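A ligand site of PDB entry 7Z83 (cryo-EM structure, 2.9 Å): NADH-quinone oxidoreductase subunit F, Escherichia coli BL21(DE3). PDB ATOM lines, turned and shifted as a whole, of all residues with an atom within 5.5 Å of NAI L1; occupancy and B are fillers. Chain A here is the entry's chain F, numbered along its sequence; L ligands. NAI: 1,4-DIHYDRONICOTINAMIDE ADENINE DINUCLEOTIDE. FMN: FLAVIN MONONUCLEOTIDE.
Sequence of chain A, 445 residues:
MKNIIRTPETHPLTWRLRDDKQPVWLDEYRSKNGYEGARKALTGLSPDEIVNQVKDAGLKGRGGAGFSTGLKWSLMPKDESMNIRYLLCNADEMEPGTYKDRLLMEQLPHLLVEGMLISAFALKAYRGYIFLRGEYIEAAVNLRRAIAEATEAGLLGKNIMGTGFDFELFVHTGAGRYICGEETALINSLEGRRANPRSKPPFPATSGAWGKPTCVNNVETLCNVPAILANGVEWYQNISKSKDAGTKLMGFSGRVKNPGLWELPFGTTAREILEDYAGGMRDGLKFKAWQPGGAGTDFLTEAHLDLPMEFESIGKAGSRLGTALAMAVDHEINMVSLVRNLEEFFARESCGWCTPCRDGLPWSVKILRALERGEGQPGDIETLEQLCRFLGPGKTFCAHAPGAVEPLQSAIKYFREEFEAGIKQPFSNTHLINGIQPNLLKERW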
ATOM      1  N   ARG A  62      28.480  -2.062   5.757  1.00  0.00           N
ATOM      2  CA  ARG A  62      27.566  -0.962   6.025  1.00  0.00           C
ATOM      3  C   ARG A  62      26.609  -1.263   7.165  1.00  0.00           C
ATOM      4  O   ARG A  62      25.732  -0.440   7.443  1.00  0.00           O
ATOM      5  CB  ARG A  62      26.772  -0.627   4.759  1.00  0.00           C
ATOM      6  CG  ARG A  62      27.634  -0.270   3.563  1.00  0.00           C
ATOM      7  CD  ARG A  62      28.527   0.906   3.884  1.00  0.00           C
ATOM      8  NE  ARG A  62      28.992   1.587   2.674  1.00  0.00           N
ATOM      9  CZ  ARG A  62      30.216   1.470   2.176  1.00  0.00           C
ATOM     10  NH1 ARG A  62      31.120   0.705   2.750  1.00  0.00           N
ATOM     11  NH2 ARG A  62      30.533   2.148   1.073  1.00  0.00           N
ATOM     12  N   GLY A  63      26.754  -2.413   7.821  1.00  0.00           N
ATOM     13  CA  GLY A  63      25.935  -2.715   8.977  1.00  0.00           C
ATOM     14  C   GLY A  63      26.197  -1.789  10.148  1.00  0.00           C
ATOM     15  O   GLY A  63      25.274  -1.445  10.895  1.00  0.00           O
ATOM     16  N   GLY A  64      27.444  -1.349  10.316  1.00  0.00           N
ATOM     17  CA  GLY A  64      27.770  -0.435  11.381  1.00  0.00           C
ATOM     18  C   GLY A  64      29.137  -0.687  11.994  1.00  0.00           C
ATOM     19  O   GLY A  64      29.619   0.122  12.796  1.00  0.00           O
ATOM     20  N   ALA A  65      29.764  -1.793  11.623  1.00  0.00           N
ATOM     21  CA  ALA A  65      31.074  -2.152  12.168  1.00  0.00           C
ATOM     22  C   ALA A  65      32.231  -1.766  11.261  1.00  0.00           C
ATOM     23  O   ALA A  65      33.335  -1.534  11.771  1.00  0.00           O
ATOM     24  CB  ALA A  65      31.135  -3.658  12.438  1.00  0.00           C
ATOM     25  N   PHE A  67      33.666  -3.655   8.902  1.00  0.00           N
ATOM     26  CA  PHE A  67      34.509  -4.773   8.501  1.00  0.00           C
ATOM     27  C   PHE A  67      34.546  -4.884   6.985  1.00  0.00           C
ATOM     28  O   PHE A  67      33.565  -4.618   6.288  1.00  0.00           O
ATOM     29  CB  PHE A  67      34.005  -6.079   9.114  1.00  0.00           C
ATOM     30  CG  PHE A  67      35.031  -7.175   9.129  1.00  0.00           C
ATOM     31  CD1 PHE A  67      36.045  -7.183  10.074  1.00  0.00           C
ATOM     32  CD2 PHE A  67      34.967  -8.211   8.216  1.00  0.00           C
ATOM     33  CE1 PHE A  67      36.988  -8.192  10.088  1.00  0.00           C
ATOM     34  CE2 PHE A  67      35.905  -9.225   8.223  1.00  0.00           C
ATOM     35  CZ  PHE A  67      36.915  -9.215   9.158  1.00  0.00           C
ATOM     36  N   LYS A  72      35.803 -10.585   4.509  1.00  0.00           N
ATOM     37  CA  LYS A  72      34.830 -11.528   5.036  1.00  0.00           C
ATOM     38  C   LYS A  72      34.458 -12.592   4.009  1.00  0.00           C
ATOM     39  O   LYS A  72      34.179 -13.740   4.371  1.00  0.00           O
ATOM     40  CB  LYS A  72      33.577 -10.783   5.489  1.00  0.00           C
ATOM     41  CG  LYS A  72      32.703 -11.570   6.456  1.00  0.00           C
ATOM     42  CD  LYS A  72      31.247 -11.153   6.339  1.00  0.00           C
ATOM     43  CE  LYS A  72      31.061  -9.708   6.756  1.00  0.00           C
ATOM     44  NZ  LYS A  72      29.636  -9.405   7.030  1.00  0.00           N
ATOM     45  N   LEU A  75      37.515 -15.543   3.627  1.00  0.00           N
ATOM     46  CA  LEU A  75      37.747 -16.594   4.601  1.00  0.00           C
ATOM     47  C   LEU A  75      36.601 -17.599   4.718  1.00  0.00           C
ATOM     48  O   LEU A  75      36.430 -18.216   5.775  1.00  0.00           O
ATOM     49  CB  LEU A  75      38.104 -15.994   5.969  1.00  0.00           C
ATOM     50  CG  LEU A  75      37.397 -14.742   6.505  1.00  0.00           C
ATOM     51  CD1 LEU A  75      35.986 -15.019   6.983  1.00  0.00           C
ATOM     52  CD2 LEU A  75      38.236 -14.135   7.616  1.00  0.00           C
ATOM     53  N   GLU A  93      17.404  -4.341  10.689  1.00  0.00           N
ATOM     54  CA  GLU A  93      17.475  -2.877  10.844  1.00  0.00           C
ATOM     55  C   GLU A  93      16.598  -2.388  12.006  1.00  0.00           C
ATOM     56  O   GLU A  93      15.766  -1.493  11.852  1.00  0.00           O
ATOM     57  CB  GLU A  93      17.103  -2.169   9.546  1.00  0.00           C
ATOM     58  CG  GLU A  93      17.803  -0.839   9.351  1.00  0.00           C
ATOM     59  CD  GLU A  93      16.984   0.133   8.536  1.00  0.00           C
ATOM     60  OE1 GLU A  93      15.742   0.036   8.548  1.00  0.00           O
ATOM     61  OE2 GLU A  93      17.586   1.015   7.877  1.00  0.00           O
ATOM     62  N   MET A  94      16.794  -2.997  13.164  1.00  0.00           N
ATOM     63  CA  MET A  94      15.979  -2.688  14.335  1.00  0.00           C
ATOM     64  C   MET A  94      16.613  -1.646  15.236  1.00  0.00           C
ATOM     65  O   MET A  94      16.066  -1.373  16.314  1.00  0.00           O
ATOM     66  CB  MET A  94      15.731  -3.972  15.132  1.00  0.00           C
ATOM     67  CG  MET A  94      14.695  -4.889  14.511  1.00  0.00           C
ATOM     68  SD  MET A  94      13.153  -4.900  15.430  1.00  0.00           S
ATOM     69  CE  MET A  94      12.382  -6.343  14.731  1.00  0.00           C
ATOM     70  N   GLU A  95      17.724  -1.062  14.829  1.00  0.00           N
ATOM     71  CA  GLU A  95      18.366  -0.017  15.625  1.00  0.00           C
ATOM     72  C   GLU A  95      17.525   1.248  15.603  1.00  0.00           C
ATOM     73  O   GLU A  95      17.070   1.671  14.529  1.00  0.00           O
ATOM     74  CB  GLU A  95      19.764   0.278  15.102  1.00  0.00           C
ATOM     75  CG  GLU A  95      20.475   1.427  15.792  1.00  0.00           C
ATOM     76  CD  GLU A  95      21.396   0.965  16.889  1.00  0.00           C
ATOM     77  OE1 GLU A  95      20.929   0.242  17.792  1.00  0.00           O
ATOM     78  OE2 GLU A  95      22.593   1.320  16.857  1.00  0.00           O
ATOM     79  N   THR A  98      17.659   4.299  12.759  1.00  0.00           N
ATOM     80  CA  THR A  98      18.106   3.738  11.487  1.00  0.00           C
ATOM     81  C   THR A  98      16.892   3.458  10.612  1.00  0.00           C
ATOM     82  O   THR A  98      15.999   2.702  11.011  1.00  0.00           O
ATOM     83  CB  THR A  98      18.919   2.468  11.699  1.00  0.00           C
ATOM     84  OG1 THR A  98      19.804   2.647  12.817  1.00  0.00           O
ATOM     85  CG2 THR A  98      19.743   2.160  10.465  1.00  0.00           C
ATOM     86  N   LYS A 100      17.591   3.557   6.840  1.00  0.00           N
ATOM     87  CA  LYS A 100      18.179   3.578   5.505  1.00  0.00           C
ATOM     88  C   LYS A 100      17.788   2.357   4.681  1.00  0.00           C
ATOM     89  O   LYS A 100      17.485   2.483   3.480  1.00  0.00           O
ATOM     90  CB  LYS A 100      19.703   3.687   5.608  1.00  0.00           C
ATOM     91  CG  LYS A 100      20.337   2.762   6.633  1.00  0.00           C
ATOM     92  CD  LYS A 100      21.833   2.945   6.691  1.00  0.00           C
ATOM     93  CE  LYS A 100      22.496   1.786   7.409  1.00  0.00           C
ATOM     94  NZ  LYS A 100      22.523   0.568   6.555  1.00  0.00           N
ATOM     95  N   TYR A 178      14.887  -7.292  18.503  1.00  0.00           N
ATOM     96  CA  TYR A 178      16.024  -6.488  18.067  1.00  0.00           C
ATOM     97  C   TYR A 178      17.314  -7.301  17.984  1.00  0.00           C
ATOM     98  O   TYR A 178      18.154  -7.027  17.125  1.00  0.00           O
ATOM     99  CB  TYR A 178      16.205  -5.304  19.021  1.00  0.00           C
ATOM    100  CG  TYR A 178      17.549  -4.594  18.953  1.00  0.00           C
ATOM    101  CD1 TYR A 178      17.801  -3.664  17.974  1.00  0.00           C
ATOM    102  CD2 TYR A 178      18.538  -4.839  19.895  1.00  0.00           C
ATOM    103  CE1 TYR A 178      19.009  -3.001  17.907  1.00  0.00           C
ATOM    104  CE2 TYR A 178      19.749  -4.194  19.838  1.00  0.00           C
ATOM    105  CZ  TYR A 178      19.978  -3.277  18.843  1.00  0.00           C
ATOM    106  OH  TYR A 178      21.180  -2.623  18.786  1.00  0.00           O
ATOM    107  N   GLU A 182      21.792  -9.255  15.090  1.00  0.00           N
ATOM    108  CA  GLU A 182      23.103  -9.863  15.286  1.00  0.00           C
ATOM    109  C   GLU A 182      23.220 -11.111  14.432  1.00  0.00           C
ATOM    110  O   GLU A 182      22.307 -11.953  14.429  1.00  0.00           O
ATOM    111  CB  GLU A 182      23.293 -10.217  16.764  1.00  0.00           C
ATOM    112  CG  GLU A 182      24.704 -10.035  17.288  1.00  0.00           C
ATOM    113  CD  GLU A 182      25.576 -11.250  17.057  1.00  0.00           C
ATOM    114  OE1 GLU A 182      25.027 -12.367  17.000  1.00  0.00           O
ATOM    115  OE2 GLU A 182      26.807 -11.079  16.932  1.00  0.00           O
ATOM    116  N   GLU A 183      24.341 -11.243  13.709  1.00  0.00           N
ATOM    117  CA  GLU A 183      24.394 -12.192  12.599  1.00  0.00           C
ATOM    118  C   GLU A 183      24.337 -13.644  13.070  1.00  0.00           C
ATOM    119  O   GLU A 183      23.741 -14.493  12.402  1.00  0.00           O
ATOM    120  CB  GLU A 183      25.642 -11.947  11.740  1.00  0.00           C
ATOM    121  CG  GLU A 183      26.947 -12.454  12.333  1.00  0.00           C
ATOM    122  CD  GLU A 183      28.136 -12.089  11.503  1.00  0.00           C
ATOM    123  OE1 GLU A 183      29.244 -12.497  11.900  1.00  0.00           O
ATOM    124  OE2 GLU A 183      27.978 -11.415  10.470  1.00  0.00           O
ATOM    125  N   LYS A 200      32.042 -16.659  18.873  1.00  0.00           N
ATOM    126  CA  LYS A 200      32.951 -16.682  17.749  1.00  0.00           C
ATOM    127  C   LYS A 200      34.378 -16.514  18.244  1.00  0.00           C
ATOM    128  O   LYS A 200      34.621 -15.636  19.082  1.00  0.00           O
ATOM    129  CB  LYS A 200      32.602 -15.566  16.743  1.00  0.00           C
ATOM    130  CG  LYS A 200      31.124 -15.527  16.367  1.00  0.00           C
ATOM    131  CD  LYS A 200      30.809 -14.332  15.494  1.00  0.00           C
ATOM    132  CE  LYS A 200      30.850 -13.032  16.285  1.00  0.00           C
ATOM    133  NZ  LYS A 200      30.311 -11.885  15.503  1.00  0.00           N
ATOM    134  N   PHE A 203      33.538 -18.523  13.224  1.00  0.00           N
ATOM    135  CA  PHE A 203      32.746 -17.500  12.578  1.00  0.00           C
ATOM    136  C   PHE A 203      31.723 -18.149  11.640  1.00  0.00           C
ATOM    137  O   PHE A 203      31.872 -19.320  11.271  1.00  0.00           O
ATOM    138  CB  PHE A 203      33.668 -16.549  11.830  1.00  0.00           C
ATOM    139  CG  PHE A 203      34.501 -15.698  12.736  1.00  0.00           C
ATOM    140  CD1 PHE A 203      33.968 -14.575  13.337  1.00  0.00           C
ATOM    141  CD2 PHE A 203      35.810 -16.049  13.023  1.00  0.00           C
ATOM    142  CE1 PHE A 203      34.732 -13.793  14.184  1.00  0.00           C
ATOM    143  CE2 PHE A 203      36.571 -15.279  13.867  1.00  0.00           C
ATOM    144  CZ  PHE A 203      36.039 -14.154  14.451  1.00  0.00           C
ATOM    145  N   PRO A 204      30.658 -17.425  11.277  1.00  0.00           N
ATOM    146  CA  PRO A 204      29.657 -18.002  10.358  1.00  0.00           C
ATOM    147  C   PRO A 204      30.207 -18.373   8.995  1.00  0.00           C
ATOM    148  O   PRO A 204      29.606 -19.228   8.320  1.00  0.00           O
ATOM    149  CB  PRO A 204      28.617 -16.887  10.256  1.00  0.00           C
ATOM    150  CG  PRO A 204      28.696 -16.204  11.552  1.00  0.00           C
ATOM    151  CD  PRO A 204      30.149 -16.197  11.914  1.00  0.00           C
ATOM    152  N   VAL A 216      26.805 -13.385   6.160  1.00  0.00           N
ATOM    153  CA  VAL A 216      25.757 -12.436   6.513  1.00  0.00           C
ATOM    154  C   VAL A 216      26.232 -11.037   6.163  1.00  0.00           C
ATOM    155  O   VAL A 216      27.322 -10.624   6.586  1.00  0.00           O
ATOM    156  CB  VAL A 216      25.395 -12.535   8.008  1.00  0.00           C
ATOM    157  CG1 VAL A 216      24.094 -11.811   8.271  1.00  0.00           C
ATOM    158  CG2 VAL A 216      25.304 -13.980   8.441  1.00  0.00           C
ATOM    159  N   ASN A 218      24.842  -6.767   5.205  1.00  0.00           N
ATOM    160  CA  ASN A 218      23.783  -5.770   5.295  1.00  0.00           C
ATOM    161  C   ASN A 218      23.178  -5.521   3.914  1.00  0.00           C
ATOM    162  O   ASN A 218      23.719  -5.902   2.872  1.00  0.00           O
ATOM    163  CB  ASN A 218      24.329  -4.473   5.889  1.00  0.00           C
ATOM    164  CG  ASN A 218      23.228  -3.553   6.397  1.00  0.00           C
ATOM    165  OD1 ASN A 218      22.082  -3.972   6.548  1.00  0.00           O
ATOM    166  ND2 ASN A 218      23.572  -2.309   6.649  1.00  0.00           N
ATOM    167  N   GLY A 293      25.595   7.383  14.986  1.00  0.00           N
ATOM    168  CA  GLY A 293      25.190   6.153  14.317  1.00  0.00           C
ATOM    169  C   GLY A 293      24.092   5.360  14.970  1.00  0.00           C
ATOM    170  O   GLY A 293      24.138   4.131  14.992  1.00  0.00           O
ATOM    171  N   ARG A 320      31.296   6.130  17.693  1.00  0.00           N
ATOM    172  CA  ARG A 320      31.348   5.231  16.549  1.00  0.00           C
ATOM    173  C   ARG A 320      30.558   5.840  15.401  1.00  0.00           C
ATOM    174  O   ARG A 320      29.571   6.552  15.620  1.00  0.00           O
ATOM    175  CB  ARG A 320      30.790   3.849  16.875  1.00  0.00           C
ATOM    176  CG  ARG A 320      31.570   3.082  17.928  1.00  0.00           C
ATOM    177  CD  ARG A 320      31.159   1.629  17.948  1.00  0.00           C
ATOM    178  NE  ARG A 320      29.889   1.418  18.645  1.00  0.00           N
ATOM    179  CZ  ARG A 320      28.719   1.263  18.045  1.00  0.00           C
ATOM    180  NH1 ARG A 320      28.605   1.325  16.727  1.00  0.00           N
ATOM    181  NH2 ARG A 320      27.637   1.051  18.780  1.00  0.00           N
ATOM    182  N   GLY A 322      28.923   3.940  13.199  1.00  0.00           N
ATOM    183  CA  GLY A 322      27.701   3.154  13.234  1.00  0.00           C
ATOM    184  C   GLY A 322      27.045   3.056  11.872  1.00  0.00           C
ATOM    185  O   GLY A 322      27.691   2.822  10.852  1.00  0.00           O
ATOM    186  N   THR A 323      25.727   3.256  11.862  1.00  0.00           N
ATOM    187  CA  THR A 323      24.962   3.276  10.623  1.00  0.00           C
ATOM    188  C   THR A 323      25.003   4.638   9.931  1.00  0.00           C
ATOM    189  O   THR A 323      24.373   4.788   8.886  1.00  0.00           O
ATOM    190  CB  THR A 323      23.505   2.899  10.892  1.00  0.00           C
ATOM    191  OG1 THR A 323      22.847   3.962  11.594  1.00  0.00           O
ATOM    192  CG2 THR A 323      23.432   1.631  11.723  1.00  0.00           C
ATOM    193  N   ALA A 399      27.744  -7.993  21.499  1.00  0.00           N
ATOM    194  CA  ALA A 399      28.019  -6.567  21.495  1.00  0.00           C
ATOM    195  C   ALA A 399      26.781  -5.706  21.691  1.00  0.00           C
ATOM    196  O   ALA A 399      26.822  -4.510  21.392  1.00  0.00           O
ATOM    197  CB  ALA A 399      28.725  -6.174  20.187  1.00  0.00           C
HETATM  198  PA  NAI L   1      32.082  -7.154  14.800  1.00  0.00           P
HETATM  199  O1A NAI L   1      32.634  -5.827  14.460  1.00  0.00           O
HETATM  200  O2A NAI L   1      33.040  -8.062  15.559  1.00  0.00           O
HETATM  201  O5B NAI L   1      31.636  -7.949  13.488  1.00  0.00           O
HETATM  202  C5B NAI L   1      31.200  -7.300  12.273  1.00  0.00           C
HETATM  203  C4B NAI L   1      31.410  -8.218  11.103  1.00  0.00           C
HETATM  204  O4B NAI L   1      32.813  -8.549  10.975  1.00  0.00           O
HETATM  205  C3B NAI L   1      30.655  -9.549  11.168  1.00  0.00           C
HETATM  206  O3B NAI L   1      30.075  -9.876   9.910  1.00  0.00           O
HETATM  207  C2B NAI L   1      31.751 -10.547  11.570  1.00  0.00           C
HETATM  208  O2B NAI L   1      31.475 -11.855  11.075  1.00  0.00           O
HETATM  209  C1B NAI L   1      32.966  -9.947  10.884  1.00  0.00           C
HETATM  210  N9A NAI L   1      34.229 -10.316  11.509  1.00  0.00           N
HETATM  211  C8A NAI L   1      34.862  -9.674  12.544  1.00  0.00           C
HETATM  212  N7A NAI L   1      35.999 -10.213  12.884  1.00  0.00           N
HETATM  213  C5A NAI L   1      36.137 -11.286  12.023  1.00  0.00           C
HETATM  214  C6A NAI L   1      37.135 -12.264  11.865  1.00  0.00           C
HETATM  215  N6A NAI L   1      38.243 -12.319  12.608  1.00  0.00           N
HETATM  216  N1A NAI L   1      36.963 -13.206  10.907  1.00  0.00           N
HETATM  217  C2A NAI L   1      35.849 -13.155  10.157  1.00  0.00           C
HETATM  218  N3A NAI L   1      34.844 -12.283  10.210  1.00  0.00           N
HETATM  219  C4A NAI L   1      35.046 -11.371  11.167  1.00  0.00           C
HETATM  220  O3  NAI L   1      30.776  -7.015  15.704  1.00  0.00           O
HETATM  221  PN  NAI L   1      29.228  -7.327  15.533  1.00  0.00           P
HETATM  222  O1N NAI L   1      28.687  -7.686  16.911  1.00  0.00           O
HETATM  223  O2N NAI L   1      28.952  -8.332  14.495  1.00  0.00           O
HETATM  224  O5D NAI L   1      28.571  -5.912  15.153  1.00  0.00           O
HETATM  225  C5D NAI L   1      28.785  -4.718  15.924  1.00  0.00           C
HETATM  226  C4D NAI L   1      28.308  -3.539  15.119  1.00  0.00           C
HETATM  227  O4D NAI L   1      26.902  -3.673  14.867  1.00  0.00           O
HETATM  228  C3D NAI L   1      28.484  -2.177  15.787  1.00  0.00           C
HETATM  229  O3D NAI L   1      29.619  -1.493  15.281  1.00  0.00           O
HETATM  230  C2D NAI L   1      27.173  -1.423  15.478  1.00  0.00           C
HETATM  231  O2D NAI L   1      27.417  -0.188  14.802  1.00  0.00           O
HETATM  232  C1D NAI L   1      26.409  -2.385  14.557  1.00  0.00           C
HETATM  233  N1N NAI L   1      24.968  -2.380  14.780  1.00  0.00           N
HETATM  234  C2N NAI L   1      24.088  -2.170  13.715  1.00  0.00           C
HETATM  235  C3N NAI L   1      22.746  -2.162  13.867  1.00  0.00           C
HETATM  236  C7N NAI L   1      21.925  -1.928  12.659  1.00  0.00           C
HETATM  237  O7N NAI L   1      22.454  -1.612  11.585  1.00  0.00           O
HETATM  238  N7N NAI L   1      20.607  -2.047  12.783  1.00  0.00           N
HETATM  239  C4N NAI L   1      22.137  -2.388  15.216  1.00  0.00           C
HETATM  240  C5N NAI L   1      23.157  -2.565  16.272  1.00  0.00           C
HETATM  241  C6N NAI L   1      24.458  -2.561  16.029  1.00  0.00           C
HETATM  242  N1  FMN L   2      23.336  -5.513  11.179  1.00  0.00           N
HETATM  243  C2  FMN L   2      22.314  -5.263  10.298  1.00  0.00           C
HETATM  244  O2  FMN L   2      22.559  -5.172   9.100  1.00  0.00           O
HETATM  245  N3  FMN L   2      21.030  -5.096  10.762  1.00  0.00           N
HETATM  246  C4  FMN L   2      20.774  -5.202  12.103  1.00  0.00           C
HETATM  247  O4  FMN L   2      19.629  -5.063  12.531  1.00  0.00           O
HETATM  248  C4A FMN L   2      21.800  -5.469  12.994  1.00  0.00           C
HETATM  249  N5  FMN L   2      21.548  -5.562  14.338  1.00  0.00           N
HETATM  250  C5A FMN L   2      22.566  -5.825  15.216  1.00  0.00           C
HETATM  251  C6  FMN L   2      22.284  -5.919  16.568  1.00  0.00           C
HETATM  252  C7  FMN L   2      23.292  -6.184  17.469  1.00  0.00           C
HETATM  253  C7M FMN L   2      22.966  -6.285  18.927  1.00  0.00           C
HETATM  254  C8  FMN L   2      24.596  -6.351  17.019  1.00  0.00           C
HETATM  255  C8M FMN L   2      25.716  -6.626  17.989  1.00  0.00           C
HETATM  256  C9  FMN L   2      24.877  -6.249  15.662  1.00  0.00           C
HETATM  257  C9A FMN L   2      23.864  -5.989  14.755  1.00  0.00           C
HETATM  258  N10 FMN L   2      24.132  -5.890  13.396  1.00  0.00           N
HETATM  259  C10 FMN L   2      23.096  -5.624  12.527  1.00  0.00           C
HETATM  260  C1' FMN L   2      25.523  -6.056  12.856  1.00  0.00           C
HETATM  261  C2' FMN L   2      25.743  -7.517  12.440  1.00  0.00           C
HETATM  262  O2' FMN L   2      26.320  -8.229  13.514  1.00  0.00           O
HETATM  263  C3' FMN L   2      26.650  -7.649  11.223  1.00  0.00           C
HETATM  264  O3' FMN L   2      27.788  -6.845  11.416  1.00  0.00           O
HETATM  265  C4' FMN L   2      25.912  -7.196   9.964  1.00  0.00           C
HETATM  266  O4' FMN L   2      24.574  -7.627  10.033  1.00  0.00           O
HETATM  267  C5' FMN L   2      26.535  -7.718   8.681  1.00  0.00           C
HETATM  268  O5' FMN L   2      27.854  -7.254   8.573  1.00  0.00           O
HETATM  269  P   FMN L   2      28.255  -6.216   7.404  1.00  0.00           P
HETATM  270  O1P FMN L   2      28.303  -4.842   8.013  1.00  0.00           O
HETATM  271  O2P FMN L   2      29.600  -6.580   6.836  1.00  0.00           O
HETATM  272  O3P FMN L   2      27.220  -6.245   6.316  1.00  0.00           O
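The backbone carbonyl oxygen of Gly 63 sits close to an oxygen (O7N) of NAI L1 (2.9 Å). CB of Ala 65 touches O1A of NAI L1, 3.3 Å away. CG of Phe 67 touches O4B of NAI L1, 3.2 Å away. CD2 of Leu 75 touches C2A of NAI L1, 3.6 Å away. CA of Glu 93 touches N7N of NAI L1 (3.8 Å). Met 94 touches NAI L1. Glu 95 touches NAI L1. Tyr 178 touches NAI L1. OE2 of Glu 182 touches O1N of NAI L1, at 3.9 Å. Phe 203 touches NAI L1. Gly 322 touches NAI L1. Thr 323 touches NAI L1. Ala 399 touches NAI L1. Hydrophobic or aromatic side chains that line NAI L1: Ala 65, Phe 67, Leu 75, Phe 203 and Ala 399. Within 4 Å of NAI L1: Gly 63, Gly 64, Ala 65, Phe 67, Lys 72, Leu 75, Glu 93, Met 94, Glu 95, Tyr 178, Glu 182, Glu 183, Lys 200, Phe 203, Arg 320, Gly 322, Thr 323 and Ala 399.
The backbone carbonyl oxygen of Gly 64 is in hydrogen-bond range of an oxygen (O3D) of NAI L1 (3.0 Å). N of Glu 93 is in hydrogen-bond range of O4 of FMN L2 (3.0 Å). OD1 of Asn 218 lies close to O2 of FMN L2 (2.9 Å). The side-chain amino group of Lys 72 lies within hydrogen-bond range of an oxygen (O3B) of NAI L1 (3.0 Å). O2D of NAI L1 lies within hydrogen-bond range of NH1 of Arg 320. O2B of NAI L1 is in hydrogen-bond range of OE1 of Glu 183, at 2.5 Å. The backbone NH (N) of Asn 218 is in hydrogen-bond range of an oxygen (O3P) of FMN L2 (2.7 Å). The backbone NH (N) of Gly 63 is in hydrogen-bond range of an oxygen (O1P) of FMN L2, 2.9 Å away. NZ of Lys 200 lies within salt-bridge range of O2N of NAI L1, at 3.9 Å. NZ of Lys 72 lies within salt-bridge range of O2P of FMN L2 (2.8 Å).
O2N of NAI L1 lies within hydrogen-bond range of O2' of FMN L2 (2.8 Å).
NZ of Lys 72 sits at hydrogen-bond distance from O of Val 216 (2.7 Å). The side-chain carboxylate (OE1) of Glu 95 lies within hydrogen-bond range of the side-chain hydroxyl (OH) of Tyr 178 (3.0 Å). OE1 of Glu 183 lies within salt-bridge range of NZ of Lys 200 (3.8 Å). OE2 of Glu 93 lies within hydrogen-bond range of N of Lys 100 (2.7 Å). OG1 of Thr 98 lies close to O of Glu 95, 3.4 Å away. The side-chain carboxylate (OE2) of Glu 182 is in salt-bridge range of the side-chain amino group (NZ) of Lys 200 (3.9 Å). ND2 of Asn 218 lies close to N of Gly 63, at 3.4 Å.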
